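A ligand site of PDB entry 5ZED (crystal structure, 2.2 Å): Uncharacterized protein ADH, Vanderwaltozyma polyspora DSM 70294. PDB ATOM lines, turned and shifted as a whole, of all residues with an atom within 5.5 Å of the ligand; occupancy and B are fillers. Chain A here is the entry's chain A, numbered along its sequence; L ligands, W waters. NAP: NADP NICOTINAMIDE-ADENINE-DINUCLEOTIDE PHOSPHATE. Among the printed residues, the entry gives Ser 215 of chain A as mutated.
NZ of Lys 36 is in salt-bridge range of O2X of the ligand, 2.7 Å away. OH of Tyr 164 is in hydrogen-bond range of O2D of the ligand (2.7 Å). The side-chain carboxylate (OE2) of Glu 56 sits at hydrogen-bond distance from a nitrogen (N6A) of the ligand (2.8 Å). N of Tyr 11 is in hydrogen-bond range of O1A of the ligand (2.8 Å). The guanidinium group (NE) of Arg 32 lies within salt-bridge range of an oxygen (O3X) of the ligand, 2.8 Å away. O3D of the ligand lies within hydrogen-bond range of O of Ala 80, 2.9 Å away. The backbone NH (N) of Ile 12 lies within hydrogen-bond range of an oxygen (O2N) of the ligand, at 2.9 Å. The side-chain amino group (NZ) of Lys 168 is in hydrogen-bond range of an oxygen (O2D) of the ligand (3.0 Å). The side-chain hydroxyl (OG) of Ser 215 lies within hydrogen-bond range of an oxygen (O7N) of the ligand. OG of Ser 9 sits at hydrogen-bond distance from O3B of the ligand (3.1 Å). A nitrogen (N1A) of the ligand lies within hydrogen-bond range of the backbone NH (N) of Ile 57 (3.1 Å). O3B of the ligand is in hydrogen-bond range of N of Gly 10, at 3.2 Å. O of Gly 7 is in hydrogen-bond range of O3B of the ligand (3.3 Å). A nitrogen (N7N) of the ligand sits close to the backbone carbonyl oxygen (O) of Ser 196, at 3.5 Å.
The side-chain carboxylate (OE1) of Glu 56 lies within salt-bridge range of the guanidinium group (NH2) of Arg 32. The side-chain carboxylate (OE2) of Glu 56 sits at hydrogen-bond distance from the backbone NH (N) of Ala 58, at 2.8 Å. NH2 of Arg 32 lies within hydrogen-bond range of O of Pro 55 (3.0 Å). The backbone carbonyl oxygen (O) of Val 198 sits at hydrogen-bond distance from the side-chain hydroxyl (OG) of Ser 215. ND2 of Asn 213 is in hydrogen-bond range of OG of Ser 215 (3.0 Å). The backbone carbonyl oxygen (O) of Pro 195 is in hydrogen-bond range of the side-chain hydroxyl (OG) of Ser 126 (3.3 Å). The backbone carbonyl oxygen of Pro 195 is in hydrogen-bond range of the backbone NH of Tyr 127 (2.8 Å). The backbone carbonyl oxygen (O) of Ser 126 sits at hydrogen-bond distance from a ring nitrogen (ND1) of His 194, at 3.1 Å.
N of Val 198 lies close to N7N of the ligand, at 2.9 Å. Residues that only touch the ligand: Pro 195 (3.2 Å), Ser 82 (3.2 Å), Ala 125 (3.2 Å), Ser 126 (3.3 Å), Phe 197 (3.4 Å), Thr 124 (3.4 Å), Pro 83 (3.5 Å), Val 84 (3.5 Å), Pro 98 (3.6 Å), Ala 81 (3.7 Å) and Asn 85 (3.96 Å). Of the 34 residues printed, 26 come within 4 Å of the ligand. Along chain A the residues within 4 Å of the ligand span positions 7 to 215. The nearest printed residue that does not touch the ligand is Asn 213 (4.02 Å).
Water W10 lies within hydrogen-bond range of OG of Ser 9 (2.6 Å) and O1X of the ligand (2.7 Å). Water W1 bridges an oxygen (O3X) of the ligand (2.7 Å) and the guanidinium group (NE) of Arg 32 (3.3 Å). Water W2 lies within hydrogen-bond range of OG of Ser 9 (2.8 Å), O2X of the ligand (2.8 Å) and N of Arg 32 (3.0 Å). Water W4 lies within hydrogen-bond range of an oxygen (O2A) of the ligand and the side-chain amide nitrogen of Asn 85. Water W7 bridges the backbone carbonyl oxygen of Gly 7 and the backbone carbonyl oxygen of Ala 80. Water W3 lies within hydrogen-bond range of NH1 of Arg 32 (3.1 Å), O of Asn 85 (3.1 Å) and N7A of the ligand (3.4 Å).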
ATOM      1  N   GLY A   7     -17.977  21.701  25.772  1.00  0.00           N
ATOM      2  CA  GLY A   7     -17.306  21.933  24.496  1.00  0.00           C
ATOM      3  C   GLY A   7     -18.060  21.372  23.312  1.00  0.00           C
ATOM      4  O   GLY A   7     -17.551  20.550  22.542  1.00  0.00           O
ATOM      5  N   ALA A   8     -19.327  21.755  23.194  1.00  0.00           N
ATOM      6  CA  ALA A   8     -20.272  21.136  22.281  1.00  0.00           C
ATOM      7  C   ALA A   8     -20.162  21.623  20.841  1.00  0.00           C
ATOM      8  O   ALA A   8     -20.930  21.144  20.009  1.00  0.00           O
ATOM      9  CB  ALA A   8     -21.699  21.367  22.806  1.00  0.00           C
ATOM     10  N   SER A   9     -19.251  22.546  20.523  1.00  0.00           N
ATOM     11  CA  SER A   9     -19.128  23.026  19.139  1.00  0.00           C
ATOM     12  C   SER A   9     -18.051  22.300  18.340  1.00  0.00           C
ATOM     13  O   SER A   9     -17.916  22.556  17.135  1.00  0.00           O
ATOM     14  CB  SER A   9     -18.837  24.528  19.135  1.00  0.00           C
ATOM     15  OG  SER A   9     -17.549  24.776  19.651  1.00  0.00           O
ATOM     16  N   GLY A  10     -17.275  21.431  18.964  1.00  0.00           N
ATOM     17  CA  GLY A  10     -16.161  20.826  18.272  1.00  0.00           C
ATOM     18  C   GLY A  10     -16.584  19.633  17.427  1.00  0.00           C
ATOM     19  O   GLY A  10     -17.734  19.189  17.417  1.00  0.00           O
ATOM     20  N   TYR A  11     -15.589  19.077  16.734  1.00  0.00           N
ATOM     21  CA  TYR A  11     -15.813  18.048  15.720  1.00  0.00           C
ATOM     22  C   TYR A  11     -16.492  16.809  16.295  1.00  0.00           C
ATOM     23  O   TYR A  11     -17.548  16.376  15.815  1.00  0.00           O
ATOM     24  CB  TYR A  11     -14.469  17.690  15.076  1.00  0.00           C
ATOM     25  CG  TYR A  11     -14.383  16.395  14.302  1.00  0.00           C
ATOM     26  CD1 TYR A  11     -13.457  15.407  14.662  1.00  0.00           C
ATOM     27  CD2 TYR A  11     -15.165  16.172  13.171  1.00  0.00           C
ATOM     28  CE1 TYR A  11     -13.322  14.216  13.928  1.00  0.00           C
ATOM     29  CE2 TYR A  11     -15.045  14.967  12.434  1.00  0.00           C
ATOM     30  CZ  TYR A  11     -14.133  14.005  12.818  1.00  0.00           C
ATOM     31  OH  TYR A  11     -14.013  12.843  12.084  1.00  0.00           O
ATOM     32  N   ILE A  12     -15.908  16.236  17.352  1.00  0.00           N
ATOM     33  CA  ILE A  12     -16.453  15.029  17.951  1.00  0.00           C
ATOM     34  C   ILE A  12     -17.750  15.327  18.683  1.00  0.00           C
ATOM     35  O   ILE A  12     -18.717  14.558  18.621  1.00  0.00           O
ATOM     36  CB  ILE A  12     -15.409  14.403  18.898  1.00  0.00           C
ATOM     37  CG1 ILE A  12     -14.182  13.923  18.123  1.00  0.00           C
ATOM     38  CG2 ILE A  12     -16.010  13.267  19.712  1.00  0.00           C
ATOM     39  CD1 ILE A  12     -12.962  13.653  19.032  1.00  0.00           C
ATOM     40  N   ALA A  13     -17.795  16.459  19.390  1.00  0.00           N
ATOM     41  CA  ALA A  13     -18.935  16.753  20.242  1.00  0.00           C
ATOM     42  C   ALA A  13     -20.217  16.873  19.414  1.00  0.00           C
ATOM     43  O   ALA A  13     -21.296  16.455  19.842  1.00  0.00           O
ATOM     44  CB  ALA A  13     -18.670  18.027  21.048  1.00  0.00           C
ATOM     45  N   ARG A  32     -18.290  28.506  23.787  1.00  0.00           N
ATOM     46  CA  ARG A  32     -17.552  29.696  24.187  1.00  0.00           C
ATOM     47  C   ARG A  32     -18.366  30.984  24.052  1.00  0.00           C
ATOM     48  O   ARG A  32     -18.172  31.916  24.842  1.00  0.00           O
ATOM     49  CB  ARG A  32     -16.285  29.804  23.337  1.00  0.00           C
ATOM     50  CG  ARG A  32     -15.150  28.833  23.693  1.00  0.00           C
ATOM     51  CD  ARG A  32     -13.811  29.563  23.669  1.00  0.00           C
ATOM     52  NE  ARG A  32     -12.664  28.707  23.408  1.00  0.00           N
ATOM     53  CZ  ARG A  32     -11.536  28.744  24.133  1.00  0.00           C
ATOM     54  NH1 ARG A  32     -10.517  27.953  23.834  1.00  0.00           N
ATOM     55  NH2 ARG A  32     -11.459  29.558  25.192  1.00  0.00           N
ATOM     56  N   LYS A  36     -21.534  31.196  18.711  1.00  0.00           N
ATOM     57  CA  LYS A  36     -21.507  29.789  18.361  1.00  0.00           C
ATOM     58  C   LYS A  36     -22.774  29.060  18.795  1.00  0.00           C
ATOM     59  O   LYS A  36     -23.230  28.154  18.094  1.00  0.00           O
ATOM     60  CB  LYS A  36     -20.253  29.125  18.943  1.00  0.00           C
ATOM     61  CG  LYS A  36     -18.969  29.705  18.327  1.00  0.00           C
ATOM     62  CD  LYS A  36     -17.737  29.558  19.197  1.00  0.00           C
ATOM     63  CE  LYS A  36     -16.471  29.638  18.352  1.00  0.00           C
ATOM     64  NZ  LYS A  36     -15.246  29.649  19.173  1.00  0.00           N
ATOM     65  N   VAL A  54     -19.819  28.982  28.346  1.00  0.00           N
ATOM     66  CA  VAL A  54     -18.602  28.875  29.142  1.00  0.00           C
ATOM     67  C   VAL A  54     -17.445  29.388  28.278  1.00  0.00           C
ATOM     68  O   VAL A  54     -16.904  28.656  27.449  1.00  0.00           O
ATOM     69  CB  VAL A  54     -18.352  27.429  29.612  1.00  0.00           C
ATOM     70  CG1 VAL A  54     -17.037  27.312  30.375  1.00  0.00           C
ATOM     71  CG2 VAL A  54     -19.499  26.961  30.493  1.00  0.00           C
ATOM     72  N   PRO A  55     -17.056  30.652  28.437  1.00  0.00           N
ATOM     73  CA  PRO A  55     -16.025  31.211  27.549  1.00  0.00           C
ATOM     74  C   PRO A  55     -14.668  30.561  27.684  1.00  0.00           C
ATOM     75  O   PRO A  55     -13.911  30.505  26.713  1.00  0.00           O
ATOM     76  CB  PRO A  55     -15.957  32.700  27.956  1.00  0.00           C
ATOM     77  CG  PRO A  55     -17.167  32.948  28.816  1.00  0.00           C
ATOM     78  CD  PRO A  55     -17.572  31.627  29.412  1.00  0.00           C
ATOM     79  N   GLU A  56     -14.332  30.054  28.858  1.00  0.00           N
ATOM     80  CA  GLU A  56     -12.958  29.578  29.065  1.00  0.00           C
ATOM     81  C   GLU A  56     -12.965  28.552  30.192  1.00  0.00           C
ATOM     82  O   GLU A  56     -13.214  28.910  31.347  1.00  0.00           O
ATOM     83  CB  GLU A  56     -12.045  30.745  29.372  1.00  0.00           C
ATOM     84  CG  GLU A  56     -10.691  30.295  29.843  1.00  0.00           C
ATOM     85  CD  GLU A  56     -10.056  29.393  28.816  1.00  0.00           C
ATOM     86  OE1 GLU A  56      -9.768  29.898  27.699  1.00  0.00           O
ATOM     87  OE2 GLU A  56      -9.857  28.196  29.114  1.00  0.00           O
ATOM     88  N   ILE A  57     -12.701  27.287  29.866  1.00  0.00           N
ATOM     89  CA  ILE A  57     -12.794  26.249  30.886  1.00  0.00           C
ATOM     90  C   ILE A  57     -11.697  26.392  31.922  1.00  0.00           C
ATOM     91  O   ILE A  57     -11.843  25.857  33.033  1.00  0.00           O
ATOM     92  CB  ILE A  57     -12.744  24.842  30.257  1.00  0.00           C
ATOM     93  CG1 ILE A  57     -11.421  24.606  29.513  1.00  0.00           C
ATOM     94  CG2 ILE A  57     -13.945  24.613  29.374  1.00  0.00           C
ATOM     95  CD1 ILE A  57     -11.431  23.262  28.761  1.00  0.00           C
ATOM     96  N   ALA A  58     -10.615  27.107  31.615  1.00  0.00           N
ATOM     97  CA  ALA A  58      -9.534  27.261  32.581  1.00  0.00           C
ATOM     98  C   ALA A  58      -9.889  28.240  33.687  1.00  0.00           C
ATOM     99  O   ALA A  58      -9.287  28.178  34.770  1.00  0.00           O
ATOM    100  CB  ALA A  58      -8.249  27.720  31.880  1.00  0.00           C
ATOM    101  N   ALA A  80     -16.102  16.859  27.352  1.00  0.00           N
ATOM    102  CA  ALA A  80     -15.370  16.708  26.115  1.00  0.00           C
ATOM    103  C   ALA A  80     -14.491  17.909  25.784  1.00  0.00           C
ATOM    104  O   ALA A  80     -13.680  17.821  24.854  1.00  0.00           O
ATOM    105  CB  ALA A  80     -16.358  16.484  24.955  1.00  0.00           C
ATOM    106  N   ALA A  81     -14.580  18.994  26.539  1.00  0.00           N
ATOM    107  CA  ALA A  81     -13.852  20.219  26.222  1.00  0.00           C
ATOM    108  C   ALA A  81     -12.402  20.106  26.676  1.00  0.00           C
ATOM    109  O   ALA A  81     -12.126  19.920  27.864  1.00  0.00           O
ATOM    110  CB  ALA A  81     -14.518  21.419  26.884  1.00  0.00           C
ATOM    111  N   SER A  82     -11.482  20.240  25.732  1.00  0.00           N
ATOM    112  CA  SER A  82     -10.056  20.304  26.023  1.00  0.00           C
ATOM    113  C   SER A  82      -9.379  20.911  24.813  1.00  0.00           C
ATOM    114  O   SER A  82      -9.874  20.738  23.683  1.00  0.00           O
ATOM    115  CB  SER A  82      -9.466  18.918  26.340  1.00  0.00           C
ATOM    116  OG  SER A  82      -8.226  19.046  27.040  1.00  0.00           O
ATOM    117  N   PRO A  83      -8.291  21.655  24.987  1.00  0.00           N
ATOM    118  CA  PRO A  83      -7.716  22.386  23.853  1.00  0.00           C
ATOM    119  C   PRO A  83      -7.069  21.456  22.835  1.00  0.00           C
ATOM    120  O   PRO A  83      -6.226  20.612  23.180  1.00  0.00           O
ATOM    121  CB  PRO A  83      -6.689  23.332  24.494  1.00  0.00           C
ATOM    122  CG  PRO A  83      -6.643  22.984  25.958  1.00  0.00           C
ATOM    123  CD  PRO A  83      -7.781  22.105  26.297  1.00  0.00           C
ATOM    124  N   VAL A  84      -7.472  21.595  21.576  1.00  0.00           N
ATOM    125  CA  VAL A  84      -6.804  20.929  20.468  1.00  0.00           C
ATOM    126  C   VAL A  84      -6.069  21.924  19.570  1.00  0.00           C
ATOM    127  O   VAL A  84      -5.061  21.560  18.965  1.00  0.00           O
ATOM    128  CB  VAL A  84      -7.808  20.084  19.649  1.00  0.00           C
ATOM    129  CG1 VAL A  84      -7.085  19.188  18.648  1.00  0.00           C
ATOM    130  CG2 VAL A  84      -8.675  19.247  20.599  1.00  0.00           C
ATOM    131  N   ASN A  85      -6.532  23.174  19.492  1.00  0.00           N
ATOM    132  CA  ASN A  85      -5.816  24.257  18.837  1.00  0.00           C
ATOM    133  C   ASN A  85      -5.173  25.122  19.906  1.00  0.00           C
ATOM    134  O   ASN A  85      -5.779  25.341  20.969  1.00  0.00           O
ATOM    135  CB  ASN A  85      -6.740  25.136  17.989  1.00  0.00           C
ATOM    136  CG  ASN A  85      -7.311  24.404  16.782  1.00  0.00           C
ATOM    137  OD1 ASN A  85      -6.573  24.029  15.868  1.00  0.00           O
ATOM    138  ND2 ASN A  85      -8.624  24.198  16.779  1.00  0.00           N
ATOM    139  N   PRO A  98      -5.651  24.818  30.598  1.00  0.00           N
ATOM    140  CA  PRO A  98      -7.079  24.619  30.360  1.00  0.00           C
ATOM    141  C   PRO A  98      -7.499  23.150  30.353  1.00  0.00           C
ATOM    142  O   PRO A  98      -8.620  22.834  30.773  1.00  0.00           O
ATOM    143  CB  PRO A  98      -7.296  25.276  28.986  1.00  0.00           C
ATOM    144  CG  PRO A  98      -6.120  26.207  28.818  1.00  0.00           C
ATOM    145  CD  PRO A  98      -5.006  25.464  29.446  1.00  0.00           C
ATOM    146  N   THR A 124     -13.820  12.714  27.745  1.00  0.00           N
ATOM    147  CA  THR A 124     -13.002  12.466  26.559  1.00  0.00           C
ATOM    148  C   THR A 124     -11.542  12.641  26.936  1.00  0.00           C
ATOM    149  O   THR A 124     -11.044  13.778  27.000  1.00  0.00           O
ATOM    150  CB  THR A 124     -13.366  13.386  25.414  1.00  0.00           C
ATOM    151  OG1 THR A 124     -14.773  13.518  25.339  1.00  0.00           O
ATOM    152  CG2 THR A 124     -12.825  12.791  24.109  1.00  0.00           C
ATOM    153  N   ALA A 125     -10.851  11.535  27.195  1.00  0.00           N
ATOM    154  CA  ALA A 125      -9.409  11.560  27.328  1.00  0.00           C
ATOM    155  C   ALA A 125      -8.837  11.393  25.930  1.00  0.00           C
ATOM    156  O   ALA A 125      -9.349  11.978  24.977  1.00  0.00           O
ATOM    157  CB  ALA A 125      -8.921  10.454  28.276  1.00  0.00           C
ATOM    158  N   SER A 126      -7.814  10.546  25.789  1.00  0.00           N
ATOM    159  CA  SER A 126      -7.267  10.278  24.475  1.00  0.00           C
ATOM    160  C   SER A 126      -6.393   9.040  24.534  1.00  0.00           C
ATOM    161  O   SER A 126      -5.819   8.709  25.580  1.00  0.00           O
ATOM    162  CB  SER A 126      -6.435  11.454  23.954  1.00  0.00           C
ATOM    163  OG  SER A 126      -5.761  11.082  22.757  1.00  0.00           O
ATOM    164  N   TYR A 127      -6.292   8.370  23.397  1.00  0.00           N
ATOM    165  CA  TYR A 127      -5.195   7.429  23.178  1.00  0.00           C
ATOM    166  C   TYR A 127      -3.874   8.011  23.637  1.00  0.00           C
ATOM    167  O   TYR A 127      -2.985   7.281  24.082  1.00  0.00           O
ATOM    168  CB  TYR A 127      -5.202   7.031  21.712  1.00  0.00           C
ATOM    169  CG  TYR A 127      -3.947   6.487  21.093  1.00  0.00           C
ATOM    170  CD1 TYR A 127      -3.568   5.150  21.277  1.00  0.00           C
ATOM    171  CD2 TYR A 127      -3.159   7.285  20.285  1.00  0.00           C
ATOM    172  CE1 TYR A 127      -2.418   4.641  20.664  1.00  0.00           C
ATOM    173  CE2 TYR A 127      -2.029   6.784  19.665  1.00  0.00           C
ATOM    174  CZ  TYR A 127      -1.652   5.461  19.856  1.00  0.00           C
ATOM    175  OH  TYR A 127      -0.511   4.975  19.247  1.00  0.00           O
ATOM    176  N   TYR A 164       0.599  18.340  23.855  1.00  0.00           N
ATOM    177  CA  TYR A 164      -0.810  18.010  23.803  1.00  0.00           C
ATOM    178  C   TYR A 164      -1.090  16.690  24.498  1.00  0.00           C
ATOM    179  O   TYR A 164      -2.043  16.584  25.280  1.00  0.00           O
ATOM    180  CB  TYR A 164      -1.297  17.960  22.349  1.00  0.00           C
ATOM    181  CG  TYR A 164      -2.663  17.290  22.239  1.00  0.00           C
ATOM    182  CD1 TYR A 164      -3.826  17.984  22.554  1.00  0.00           C
ATOM    183  CD2 TYR A 164      -2.768  15.954  21.838  1.00  0.00           C
ATOM    184  CE1 TYR A 164      -5.059  17.389  22.471  1.00  0.00           C
ATOM    185  CE2 TYR A 164      -4.029  15.332  21.751  1.00  0.00           C
ATOM    186  CZ  TYR A 164      -5.163  16.067  22.068  1.00  0.00           C
ATOM    187  OH  TYR A 164      -6.410  15.499  22.007  1.00  0.00           O
ATOM    188  N   LYS A 168      -3.545  15.881  27.816  1.00  0.00           N
ATOM    189  CA  LYS A 168      -4.584  14.875  28.015  1.00  0.00           C
ATOM    190  C   LYS A 168      -4.250  13.968  29.191  1.00  0.00           C
ATOM    191  O   LYS A 168      -5.140  13.584  29.953  1.00  0.00           O
ATOM    192  CB  LYS A 168      -4.792  14.052  26.750  1.00  0.00           C
ATOM    193  CG  LYS A 168      -5.101  14.895  25.539  1.00  0.00           C
ATOM    194  CD  LYS A 168      -6.425  15.595  25.648  1.00  0.00           C
ATOM    195  CE  LYS A 168      -7.580  14.637  25.742  1.00  0.00           C
ATOM    196  NZ  LYS A 168      -8.825  15.325  26.182  1.00  0.00           N
ATOM    197  N   HIS A 194     -10.850   7.044  25.130  1.00  0.00           N
ATOM    198  CA  HIS A 194      -9.495   7.302  24.640  1.00  0.00           C
ATOM    199  C   HIS A 194      -9.416   7.094  23.136  1.00  0.00           C
ATOM    200  O   HIS A 194      -8.897   6.061  22.678  1.00  0.00           O
ATOM    201  CB  HIS A 194      -8.472   6.437  25.378  1.00  0.00           C
ATOM    202  CG  HIS A 194      -8.556   6.536  26.867  1.00  0.00           C
ATOM    203  ND1 HIS A 194      -7.588   7.167  27.626  1.00  0.00           N
ATOM    204  CD2 HIS A 194      -9.496   6.101  27.750  1.00  0.00           C
ATOM    205  CE1 HIS A 194      -7.928   7.111  28.907  1.00  0.00           C
ATOM    206  NE2 HIS A 194      -9.083   6.484  29.010  1.00  0.00           N
ATOM    207  N   PRO A 195      -9.917   8.022  22.330  1.00  0.00           N
ATOM    208  CA  PRO A 195      -9.764   7.876  20.880  1.00  0.00           C
ATOM    209  C   PRO A 195      -8.331   8.117  20.447  1.00  0.00           C
ATOM    210  O   PRO A 195      -7.606   8.938  21.009  1.00  0.00           O
ATOM    211  CB  PRO A 195     -10.700   8.946  20.302  1.00  0.00           C
ATOM    212  CG  PRO A 195     -11.496   9.491  21.467  1.00  0.00           C
ATOM    213  CD  PRO A 195     -10.632   9.258  22.687  1.00  0.00           C
ATOM    214  N   SER A 196      -7.917   7.370  19.426  1.00  0.00           N
ATOM    215  CA  SER A 196      -6.721   7.751  18.700  1.00  0.00           C
ATOM    216  C   SER A 196      -7.123   8.797  17.661  1.00  0.00           C
ATOM    217  O   SER A 196      -8.115   9.501  17.866  1.00  0.00           O
ATOM    218  CB  SER A 196      -6.065   6.492  18.119  1.00  0.00           C
ATOM    219  OG  SER A 196      -6.997   5.707  17.385  1.00  0.00           O
ATOM    220  N   PHE A 197      -6.379   8.956  16.587  1.00  0.00           N
ATOM    221  CA  PHE A 197      -6.717  10.036  15.655  1.00  0.00           C
ATOM    222  C   PHE A 197      -8.105   9.802  15.055  1.00  0.00           C
ATOM    223  O   PHE A 197      -8.372   8.743  14.487  1.00  0.00           O
ATOM    224  CB  PHE A 197      -5.664  10.125  14.556  1.00  0.00           C
ATOM    225  CG  PHE A 197      -4.453  10.852  14.992  1.00  0.00           C
ATOM    226  CD1 PHE A 197      -4.325  12.211  14.741  1.00  0.00           C
ATOM    227  CD2 PHE A 197      -3.450  10.202  15.677  1.00  0.00           C
ATOM    228  CE1 PHE A 197      -3.199  12.901  15.137  1.00  0.00           C
ATOM    229  CE2 PHE A 197      -2.308  10.876  16.070  1.00  0.00           C
ATOM    230  CZ  PHE A 197      -2.182  12.225  15.799  1.00  0.00           C
ATOM    231  N   VAL A 198      -8.982  10.786  15.206  1.00  0.00           N
ATOM    232  CA  VAL A 198     -10.391  10.594  14.878  1.00  0.00           C
ATOM    233  C   VAL A 198     -10.635  11.110  13.465  1.00  0.00           C
ATOM    234  O   VAL A 198     -10.369  12.275  13.161  1.00  0.00           O
ATOM    235  CB  VAL A 198     -11.305  11.294  15.897  1.00  0.00           C
ATOM    236  CG1 VAL A 198     -12.749  11.078  15.489  1.00  0.00           C
ATOM    237  CG2 VAL A 198     -11.035  10.807  17.323  1.00  0.00           C
ATOM    238  N   ASN A 213     -10.883  20.697  11.621  1.00  0.00           N
ATOM    239  CA  ASN A 213     -10.290  20.358  12.905  1.00  0.00           C
ATOM    240  C   ASN A 213      -9.010  19.546  12.697  1.00  0.00           C
ATOM    241  O   ASN A 213      -8.854  18.876  11.672  1.00  0.00           O
ATOM    242  CB  ASN A 213     -11.275  19.545  13.732  1.00  0.00           C
ATOM    243  CG  ASN A 213     -11.643  18.244  13.048  1.00  0.00           C
ATOM    244  OD1 ASN A 213     -12.440  18.224  12.122  1.00  0.00           O
ATOM    245  ND2 ASN A 213     -11.052  17.139  13.519  1.00  0.00           N
ATOM    246  N   SER A 215      -7.484  16.715  13.579  1.00  0.00           N
ATOM    247  CA  SER A 215      -7.346  15.320  13.154  1.00  0.00           C
ATOM    248  C   SER A 215      -7.767  15.145  11.699  1.00  0.00           C
ATOM    249  O   SER A 215      -7.018  14.570  10.894  1.00  0.00           O
ATOM    250  CB  SER A 215      -8.109  14.377  14.099  1.00  0.00           C
ATOM    251  OG  SER A 215      -9.527  14.594  14.112  1.00  0.00           O
HETATM  252  PA  NAP L   1     -12.265  20.488  18.298  1.00  0.00           P
HETATM  253  O1A NAP L   1     -13.218  20.461  17.126  1.00  0.00           O
HETATM  254  O2A NAP L   1     -11.238  21.591  18.216  1.00  0.00           O
HETATM  255  O5B NAP L   1     -13.161  20.632  19.668  1.00  0.00           O
HETATM  256  C5B NAP L   1     -12.592  21.096  20.855  1.00  0.00           C
HETATM  257  C4B NAP L   1     -13.774  21.588  21.726  1.00  0.00           C
HETATM  258  O4B NAP L   1     -13.386  21.916  22.946  1.00  0.00           O
HETATM  259  C3B NAP L   1     -14.310  22.863  21.073  1.00  0.00           C
HETATM  260  O3B NAP L   1     -15.661  22.971  21.282  1.00  0.00           O
HETATM  261  C2B NAP L   1     -13.540  23.941  21.838  1.00  0.00           C
HETATM  262  O2B NAP L   1     -14.320  25.189  21.636  1.00  0.00           O
HETATM  263  C1B NAP L   1     -13.556  23.514  23.086  1.00  0.00           C
HETATM  264  N9A NAP L   1     -12.397  23.983  23.791  1.00  0.00           N
HETATM  265  C8A NAP L   1     -11.090  23.720  23.679  1.00  0.00           C
HETATM  266  N7A NAP L   1     -10.443  24.456  24.602  1.00  0.00           N
HETATM  267  C5A NAP L   1     -11.353  25.170  25.283  1.00  0.00           C
HETATM  268  C6A NAP L   1     -11.221  26.091  26.309  1.00  0.00           C
HETATM  269  N6A NAP L   1      -9.979  26.500  26.932  1.00  0.00           N
HETATM  270  N1A NAP L   1     -12.287  26.682  26.838  1.00  0.00           N
HETATM  271  C2A NAP L   1     -13.526  26.384  26.335  1.00  0.00           C
HETATM  272  N3A NAP L   1     -13.659  25.507  25.312  1.00  0.00           N
HETATM  273  C4A NAP L   1     -12.565  24.885  24.785  1.00  0.00           C
HETATM  274  O3  NAP L   1     -11.410  19.109  18.365  1.00  0.00           O
HETATM  275  PN  NAP L   1     -12.017  17.595  18.616  1.00  0.00           P
HETATM  276  O1N NAP L   1     -11.268  16.746  17.604  1.00  0.00           O
HETATM  277  O2N NAP L   1     -13.520  17.520  18.462  1.00  0.00           O
HETATM  278  O5D NAP L   1     -11.687  17.177  20.142  1.00  0.00           O
HETATM  279  C5D NAP L   1     -12.738  17.168  21.060  1.00  0.00           C
HETATM  280  C4D NAP L   1     -12.256  16.321  22.259  1.00  0.00           C
HETATM  281  O4D NAP L   1     -11.876  15.140  21.816  1.00  0.00           O
HETATM  282  C3D NAP L   1     -11.003  16.962  22.900  1.00  0.00           C
HETATM  283  O3D NAP L   1     -11.055  16.816  24.248  1.00  0.00           O
HETATM  284  C2D NAP L   1      -9.841  16.117  22.335  1.00  0.00           C
HETATM  285  O2D NAP L   1      -8.677  16.190  23.265  1.00  0.00           O
HETATM  286  C1D NAP L   1     -10.374  14.909  22.315  1.00  0.00           C
HETATM  287  N1N NAP L   1      -9.719  14.029  21.397  1.00  0.00           N
HETATM  288  C2N NAP L   1      -9.731  14.281  20.064  1.00  0.00           C
HETATM  289  C3N NAP L   1      -9.097  13.398  19.214  1.00  0.00           C
HETATM  290  C7N NAP L   1      -9.035  13.627  17.707  1.00  0.00           C
HETATM  291  O7N NAP L   1      -9.729  14.416  17.152  1.00  0.00           O
HETATM  292  N7N NAP L   1      -8.074  12.853  16.977  1.00  0.00           N
HETATM  293  C4N NAP L   1      -8.461  12.301  19.708  1.00  0.00           C
HETATM  294  C5N NAP L   1      -8.463  12.036  21.038  1.00  0.00           C
HETATM  295  C6N NAP L   1      -9.109  12.929  21.904  1.00  0.00           C
HETATM  296  P2B NAP L   1     -13.688  26.372  20.666  1.00  0.00           P
HETATM  297  O1X NAP L   1     -13.441  25.873  19.291  1.00  0.00           O
HETATM  298  O2X NAP L   1     -14.700  27.491  20.628  1.00  0.00           O
HETATM  299  O3X NAP L   1     -12.415  26.908  21.288  1.00  0.00           O
HETATM  300  O   HOH W   1     -11.662  29.373  20.363  1.00  0.00           O
HETATM  301  O   HOH W   2     -17.194  26.676  21.646  1.00  0.00           O
HETATM  302  O   HOH W   3      -8.255  26.187  22.667  1.00  0.00           O
HETATM  303  O   HOH W   4      -9.067  20.839  16.328  1.00  0.00           O
HETATM  304  O   HOH W   5     -15.578  18.198  20.037  1.00  0.00           O
HETATM  305  O   HOH W   6     -16.576  25.266  24.149  1.00  0.00           O
HETATM  306  O   HOH W   7     -15.411  18.867  22.645  1.00  0.00           O
HETATM  307  O   HOH W   8      -9.325  17.664  16.080  1.00  0.00           O
HETATM  308  O   HOH W   9      -9.448  23.215  20.488  1.00  0.00           O
HETATM  309  O   HOH W  10     -15.573  24.993  17.947  1.00  0.00           O
HETATM  310  O   HOH W  11     -13.695  22.019  14.799  1.00  0.00           O
